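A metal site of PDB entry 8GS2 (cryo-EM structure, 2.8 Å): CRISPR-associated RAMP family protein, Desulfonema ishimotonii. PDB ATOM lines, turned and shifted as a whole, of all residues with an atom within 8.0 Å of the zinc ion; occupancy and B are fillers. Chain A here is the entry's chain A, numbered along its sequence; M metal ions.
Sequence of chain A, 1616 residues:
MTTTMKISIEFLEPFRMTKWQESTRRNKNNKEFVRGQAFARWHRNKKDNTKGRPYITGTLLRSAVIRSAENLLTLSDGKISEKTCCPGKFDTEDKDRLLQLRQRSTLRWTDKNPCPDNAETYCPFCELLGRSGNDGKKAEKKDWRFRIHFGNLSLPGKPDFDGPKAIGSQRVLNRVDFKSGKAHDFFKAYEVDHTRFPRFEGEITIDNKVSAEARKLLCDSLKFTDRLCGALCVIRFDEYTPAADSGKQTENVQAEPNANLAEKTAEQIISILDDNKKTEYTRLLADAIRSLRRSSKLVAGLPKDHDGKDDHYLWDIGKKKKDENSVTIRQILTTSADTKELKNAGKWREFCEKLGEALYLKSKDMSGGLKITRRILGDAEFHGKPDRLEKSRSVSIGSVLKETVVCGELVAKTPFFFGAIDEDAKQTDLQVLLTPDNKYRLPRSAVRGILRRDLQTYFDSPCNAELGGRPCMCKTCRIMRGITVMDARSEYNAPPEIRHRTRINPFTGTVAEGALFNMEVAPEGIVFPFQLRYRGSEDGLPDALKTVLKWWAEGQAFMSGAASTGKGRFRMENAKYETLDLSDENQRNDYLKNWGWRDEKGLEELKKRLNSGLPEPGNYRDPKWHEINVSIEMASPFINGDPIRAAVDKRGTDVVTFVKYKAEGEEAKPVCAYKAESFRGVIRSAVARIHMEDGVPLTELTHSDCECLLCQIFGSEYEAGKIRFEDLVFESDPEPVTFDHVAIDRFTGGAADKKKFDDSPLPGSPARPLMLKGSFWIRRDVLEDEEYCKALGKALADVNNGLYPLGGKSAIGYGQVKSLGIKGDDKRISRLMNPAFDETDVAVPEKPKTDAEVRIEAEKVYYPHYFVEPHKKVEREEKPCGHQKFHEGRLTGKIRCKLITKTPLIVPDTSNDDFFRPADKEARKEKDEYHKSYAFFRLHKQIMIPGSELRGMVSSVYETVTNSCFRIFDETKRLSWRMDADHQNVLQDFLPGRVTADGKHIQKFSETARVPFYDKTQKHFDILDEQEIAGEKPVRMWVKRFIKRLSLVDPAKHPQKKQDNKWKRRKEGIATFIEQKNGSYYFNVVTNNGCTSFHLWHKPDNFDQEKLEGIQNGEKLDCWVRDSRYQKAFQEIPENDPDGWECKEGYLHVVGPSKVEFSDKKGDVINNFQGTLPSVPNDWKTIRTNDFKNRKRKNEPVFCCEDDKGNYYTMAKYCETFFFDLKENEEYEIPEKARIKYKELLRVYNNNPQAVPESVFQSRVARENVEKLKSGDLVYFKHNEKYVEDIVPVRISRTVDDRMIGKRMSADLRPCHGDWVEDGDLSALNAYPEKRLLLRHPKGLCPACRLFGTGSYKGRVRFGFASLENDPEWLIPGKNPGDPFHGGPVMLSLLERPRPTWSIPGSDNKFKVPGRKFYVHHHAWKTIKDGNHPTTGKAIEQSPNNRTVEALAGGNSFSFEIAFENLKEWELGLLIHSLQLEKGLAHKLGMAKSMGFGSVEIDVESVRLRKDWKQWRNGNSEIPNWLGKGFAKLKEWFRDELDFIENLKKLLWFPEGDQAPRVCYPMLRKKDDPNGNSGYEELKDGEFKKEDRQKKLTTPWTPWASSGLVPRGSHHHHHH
Of the 18 residues printed, 4 come within 4 Å of the zinc ion. The nearest printed residue that does not touch the zinc ion is Ala 465 (4.6 Å).
SG of Cys 477 binds the zinc ion (2.3 Å). SG of Cys 463 is bound to the zinc ion, 2.3 Å away. The zinc ion is bound by SG of Cys 474. SG of Cys 472 is bound to the zinc ion, 2.3 Å away. The zinc ion has four donor atoms within binding distance.
The side-chain sulfur (SG) of Cys 477 lies close to the guanidinium group (NH1) of Arg 452, at 3.3 Å. The side-chain amide oxygen (OE1) of Gln 456 lies within hydrogen-bond range of the backbone NH (N) of Cys 463 (2.7 Å). N of Thr 476 lies close to SG of Cys 474. The guanidinium group (NH1) of Arg 481 sits at hydrogen-bond distance from the backbone carbonyl oxygen (O) of Cys 472, 2.4 Å away.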
ATOM      1  N   ARG A 452       0.900 -13.909 -38.085  1.00  0.00           N
ATOM      2  CA  ARG A 452       1.162 -14.711 -36.885  1.00  0.00           C
ATOM      3  C   ARG A 452       2.157 -15.825 -37.182  1.00  0.00           C
ATOM      4  O   ARG A 452       3.058 -16.099 -36.382  1.00  0.00           O
ATOM      5  CB  ARG A 452      -0.148 -15.279 -36.347  1.00  0.00           C
ATOM      6  CG  ARG A 452       0.005 -16.123 -35.095  1.00  0.00           C
ATOM      7  CD  ARG A 452      -1.335 -16.661 -34.630  1.00  0.00           C
ATOM      8  NE  ARG A 452      -2.227 -15.592 -34.208  1.00  0.00           N
ATOM      9  CZ  ARG A 452      -2.292 -15.108 -32.979  1.00  0.00           C
ATOM     10  NH1 ARG A 452      -1.502 -15.558 -32.018  1.00  0.00           N
ATOM     11  NH2 ARG A 452      -3.160 -14.142 -32.704  1.00  0.00           N
ATOM     12  N   GLN A 456       5.827 -16.186 -35.410  1.00  0.00           N
ATOM     13  CA  GLN A 456       6.270 -17.407 -34.749  1.00  0.00           C
ATOM     14  C   GLN A 456       7.535 -17.969 -35.384  1.00  0.00           C
ATOM     15  O   GLN A 456       8.393 -18.518 -34.678  1.00  0.00           O
ATOM     16  CB  GLN A 456       5.158 -18.456 -34.764  1.00  0.00           C
ATOM     17  CG  GLN A 456       3.947 -18.084 -33.925  1.00  0.00           C
ATOM     18  CD  GLN A 456       2.870 -19.139 -33.993  1.00  0.00           C
ATOM     19  OE1 GLN A 456       2.801 -20.028 -33.141  1.00  0.00           O
ATOM     20  NE2 GLN A 456       2.012 -19.043 -34.993  1.00  0.00           N
ATOM     21  N   SER A 461       9.452 -20.086 -31.898  1.00  0.00           N
ATOM     22  CA  SER A 461       8.747 -20.642 -30.742  1.00  0.00           C
ATOM     23  C   SER A 461       7.267 -20.714 -31.054  1.00  0.00           C
ATOM     24  O   SER A 461       6.581 -19.677 -31.023  1.00  0.00           O
ATOM     25  CB  SER A 461       8.994 -19.811 -29.492  1.00  0.00           C
ATOM     26  OG  SER A 461       8.536 -18.487 -29.660  1.00  0.00           O
ATOM     27  N   PRO A 462       6.727 -21.895 -31.364  1.00  0.00           N
ATOM     28  CA  PRO A 462       5.292 -22.006 -31.650  1.00  0.00           C
ATOM     29  C   PRO A 462       4.464 -21.642 -30.428  1.00  0.00           C
ATOM     30  O   PRO A 462       4.860 -21.863 -29.287  1.00  0.00           O
ATOM     31  CB  PRO A 462       5.108 -23.482 -32.028  1.00  0.00           C
ATOM     32  CG  PRO A 462       6.480 -23.945 -32.415  1.00  0.00           C
ATOM     33  CD  PRO A 462       7.422 -23.176 -31.557  1.00  0.00           C
ATOM     34  N   CYS A 463       3.285 -21.088 -30.687  1.00  0.00           N
ATOM     35  CA  CYS A 463       2.335 -20.740 -29.631  1.00  0.00           C
ATOM     36  C   CYS A 463       1.387 -21.912 -29.439  1.00  0.00           C
ATOM     37  O   CYS A 463       0.445 -22.108 -30.224  1.00  0.00           O
ATOM     38  CB  CYS A 463       1.583 -19.458 -29.979  1.00  0.00           C
ATOM     39  SG  CYS A 463       0.317 -19.023 -28.769  1.00  0.00           S
ATOM     40  N   ASN A 464       1.634 -22.712 -28.405  1.00  0.00           N
ATOM     41  CA  ASN A 464       0.799 -23.875 -28.114  1.00  0.00           C
ATOM     42  C   ASN A 464      -0.339 -23.501 -27.161  1.00  0.00           C
ATOM     43  O   ASN A 464      -0.459 -24.013 -26.052  1.00  0.00           O
ATOM     44  CB  ASN A 464       1.661 -25.000 -27.540  1.00  0.00           C
ATOM     45  CG  ASN A 464       2.704 -25.500 -28.524  1.00  0.00           C
ATOM     46  OD1 ASN A 464       2.461 -25.559 -29.730  1.00  0.00           O
ATOM     47  ND2 ASN A 464       3.871 -25.849 -28.017  1.00  0.00           N
ATOM     48  N   ALA A 465      -1.170 -22.583 -27.636  1.00  0.00           N
ATOM     49  CA  ALA A 465      -2.322 -22.111 -26.886  1.00  0.00           C
ATOM     50  C   ALA A 465      -3.606 -22.683 -27.473  1.00  0.00           C
ATOM     51  O   ALA A 465      -3.629 -23.181 -28.600  1.00  0.00           O
ATOM     52  CB  ALA A 465      -2.386 -20.580 -26.893  1.00  0.00           C
ATOM     53  N   GLU A 466      -4.666 -22.611 -26.675  1.00  0.00           N
ATOM     54  CA  GLU A 466      -5.969 -23.122 -27.066  1.00  0.00           C
ATOM     55  C   GLU A 466      -7.013 -22.022 -26.930  1.00  0.00           C
ATOM     56  O   GLU A 466      -6.876 -21.109 -26.114  1.00  0.00           O
ATOM     57  CB  GLU A 466      -6.365 -24.337 -26.208  1.00  0.00           C
ATOM     58  CG  GLU A 466      -7.646 -25.042 -26.628  1.00  0.00           C
ATOM     59  CD  GLU A 466      -7.559 -25.632 -28.026  1.00  0.00           C
ATOM     60  OE1 GLU A 466      -6.431 -25.976 -28.465  1.00  0.00           O
ATOM     61  OE2 GLU A 466      -8.605 -25.751 -28.689  1.00  0.00           O
ATOM     62  N   PRO A 471      -6.175 -14.237 -21.972  1.00  0.00           N
ATOM     63  CA  PRO A 471      -5.343 -14.042 -23.160  1.00  0.00           C
ATOM     64  C   PRO A 471      -3.936 -14.609 -22.984  1.00  0.00           C
ATOM     65  O   PRO A 471      -3.352 -14.544 -21.911  1.00  0.00           O
ATOM     66  CB  PRO A 471      -5.306 -12.516 -23.309  1.00  0.00           C
ATOM     67  CG  PRO A 471      -6.551 -12.052 -22.652  1.00  0.00           C
ATOM     68  CD  PRO A 471      -6.769 -12.981 -21.499  1.00  0.00           C
ATOM     69  N   CYS A 472      -3.414 -15.176 -24.066  1.00  0.00           N
ATOM     70  CA  CYS A 472      -2.063 -15.700 -24.059  1.00  0.00           C
ATOM     71  C   CYS A 472      -1.047 -14.577 -23.923  1.00  0.00           C
ATOM     72  O   CYS A 472      -1.200 -13.503 -24.525  1.00  0.00           O
ATOM     73  CB  CYS A 472      -1.789 -16.498 -25.334  1.00  0.00           C
ATOM     74  SG  CYS A 472      -0.148 -17.232 -25.434  1.00  0.00           S
ATOM     75  N   MET A 473      -0.012 -14.809 -23.133  1.00  0.00           N
ATOM     76  CA  MET A 473       0.994 -13.791 -22.832  1.00  0.00           C
ATOM     77  C   MET A 473       2.300 -14.012 -23.583  1.00  0.00           C
ATOM     78  O   MET A 473       3.315 -13.391 -23.252  1.00  0.00           O
ATOM     79  CB  MET A 473       1.251 -13.739 -21.323  1.00  0.00           C
ATOM     80  CG  MET A 473       0.020 -13.402 -20.506  1.00  0.00           C
ATOM     81  SD  MET A 473      -0.771 -11.874 -21.024  1.00  0.00           S
ATOM     82  CE  MET A 473       0.587 -10.720 -20.857  1.00  0.00           C
ATOM     83  N   CYS A 474       2.301 -14.884 -24.590  1.00  0.00           N
ATOM     84  CA  CYS A 474       3.498 -15.067 -25.387  1.00  0.00           C
ATOM     85  C   CYS A 474       3.733 -13.830 -26.257  1.00  0.00           C
ATOM     86  O   CYS A 474       2.825 -13.045 -26.533  1.00  0.00           O
ATOM     87  CB  CYS A 474       3.400 -16.315 -26.255  1.00  0.00           C
ATOM     88  SG  CYS A 474       2.563 -16.090 -27.835  1.00  0.00           S
ATOM     89  N   LYS A 475       4.985 -13.665 -26.684  1.00  0.00           N
ATOM     90  CA  LYS A 475       5.369 -12.458 -27.413  1.00  0.00           C
ATOM     91  C   LYS A 475       4.624 -12.332 -28.736  1.00  0.00           C
ATOM     92  O   LYS A 475       4.239 -11.220 -29.126  1.00  0.00           O
ATOM     93  CB  LYS A 475       6.882 -12.439 -27.642  1.00  0.00           C
ATOM     94  CG  LYS A 475       7.519 -13.823 -27.623  1.00  0.00           C
ATOM     95  CD  LYS A 475       9.026 -13.740 -27.505  1.00  0.00           C
ATOM     96  CE  LYS A 475       9.656 -15.120 -27.464  1.00  0.00           C
ATOM     97  NZ  LYS A 475      11.130 -15.075 -27.374  1.00  0.00           N
ATOM     98  N   THR A 476       4.406 -13.448 -29.440  1.00  0.00           N
ATOM     99  CA  THR A 476       3.659 -13.397 -30.692  1.00  0.00           C
ATOM    100  C   THR A 476       2.235 -12.915 -30.474  1.00  0.00           C
ATOM    101  O   THR A 476       1.740 -12.052 -31.211  1.00  0.00           O
ATOM    102  CB  THR A 476       3.672 -14.766 -31.365  1.00  0.00           C
ATOM    103  OG1 THR A 476       5.015 -15.199 -31.571  1.00  0.00           O
ATOM    104  CG2 THR A 476       2.960 -14.714 -32.698  1.00  0.00           C
ATOM    105  N   CYS A 477       1.563 -13.459 -29.454  1.00  0.00           N
ATOM    106  CA  CYS A 477       0.196 -13.023 -29.160  1.00  0.00           C
ATOM    107  C   CYS A 477       0.155 -11.578 -28.672  1.00  0.00           C
ATOM    108  O   CYS A 477      -0.780 -10.840 -29.009  1.00  0.00           O
ATOM    109  CB  CYS A 477      -0.443 -13.943 -28.128  1.00  0.00           C
ATOM    110  SG  CYS A 477      -1.025 -15.518 -28.783  1.00  0.00           S
ATOM    111  N   ARG A 478       1.149 -11.167 -27.879  1.00  0.00           N
ATOM    112  CA  ARG A 478       1.204  -9.774 -27.442  1.00  0.00           C
ATOM    113  C   ARG A 478       1.351  -8.829 -28.625  1.00  0.00           C
ATOM    114  O   ARG A 478       0.705  -7.773 -28.663  1.00  0.00           O
ATOM    115  CB  ARG A 478       2.360  -9.579 -26.455  1.00  0.00           C
ATOM    116  CG  ARG A 478       2.069 -10.084 -25.056  1.00  0.00           C
ATOM    117  CD  ARG A 478       3.230  -9.759 -24.127  1.00  0.00           C
ATOM    118  NE  ARG A 478       4.387 -10.598 -24.407  1.00  0.00           N
ATOM    119  CZ  ARG A 478       5.626 -10.305 -24.031  1.00  0.00           C
ATOM    120  NH1 ARG A 478       5.911  -9.186 -23.393  1.00  0.00           N
ATOM    121  NH2 ARG A 478       6.611 -11.166 -24.317  1.00  0.00           N
ATOM    122  N   MET A 480       0.393  -9.533 -31.748  1.00  0.00           N
ATOM    123  CA  MET A 480      -0.790  -9.639 -32.592  1.00  0.00           C
ATOM    124  C   MET A 480      -1.985  -8.911 -31.981  1.00  0.00           C
ATOM    125  O   MET A 480      -2.842  -8.429 -32.730  1.00  0.00           O
ATOM    126  CB  MET A 480      -1.146 -11.105 -32.839  1.00  0.00           C
ATOM    127  CG  MET A 480      -0.150 -11.836 -33.727  1.00  0.00           C
ATOM    128  SD  MET A 480       0.026 -11.082 -35.350  1.00  0.00           S
ATOM    129  CE  MET A 480      -1.634 -11.227 -35.984  1.00  0.00           C
ATOM    130  N   ARG A 481      -2.066  -8.823 -30.656  1.00  0.00           N
ATOM    131  CA  ARG A 481      -3.183  -8.116 -30.037  1.00  0.00           C
ATOM    132  C   ARG A 481      -3.153  -6.613 -30.314  1.00  0.00           C
ATOM    133  O   ARG A 481      -4.173  -5.950 -30.113  1.00  0.00           O
ATOM    134  CB  ARG A 481      -3.207  -8.370 -28.535  1.00  0.00           C
ATOM    135  CG  ARG A 481      -3.771  -9.726 -28.151  1.00  0.00           C
ATOM    136  CD  ARG A 481      -4.211  -9.765 -26.696  1.00  0.00           C
ATOM    137  NE  ARG A 481      -3.101  -9.559 -25.777  1.00  0.00           N
ATOM    138  CZ  ARG A 481      -2.371 -10.530 -25.245  1.00  0.00           C
ATOM    139  NH1 ARG A 481      -2.609 -11.796 -25.526  1.00  0.00           N
ATOM    140  NH2 ARG A 481      -1.377 -10.224 -24.410  1.00  0.00           N
HETATM  141 ZN    ZN M   1       0.412 -16.970 -27.684  1.00  0.00          ZN
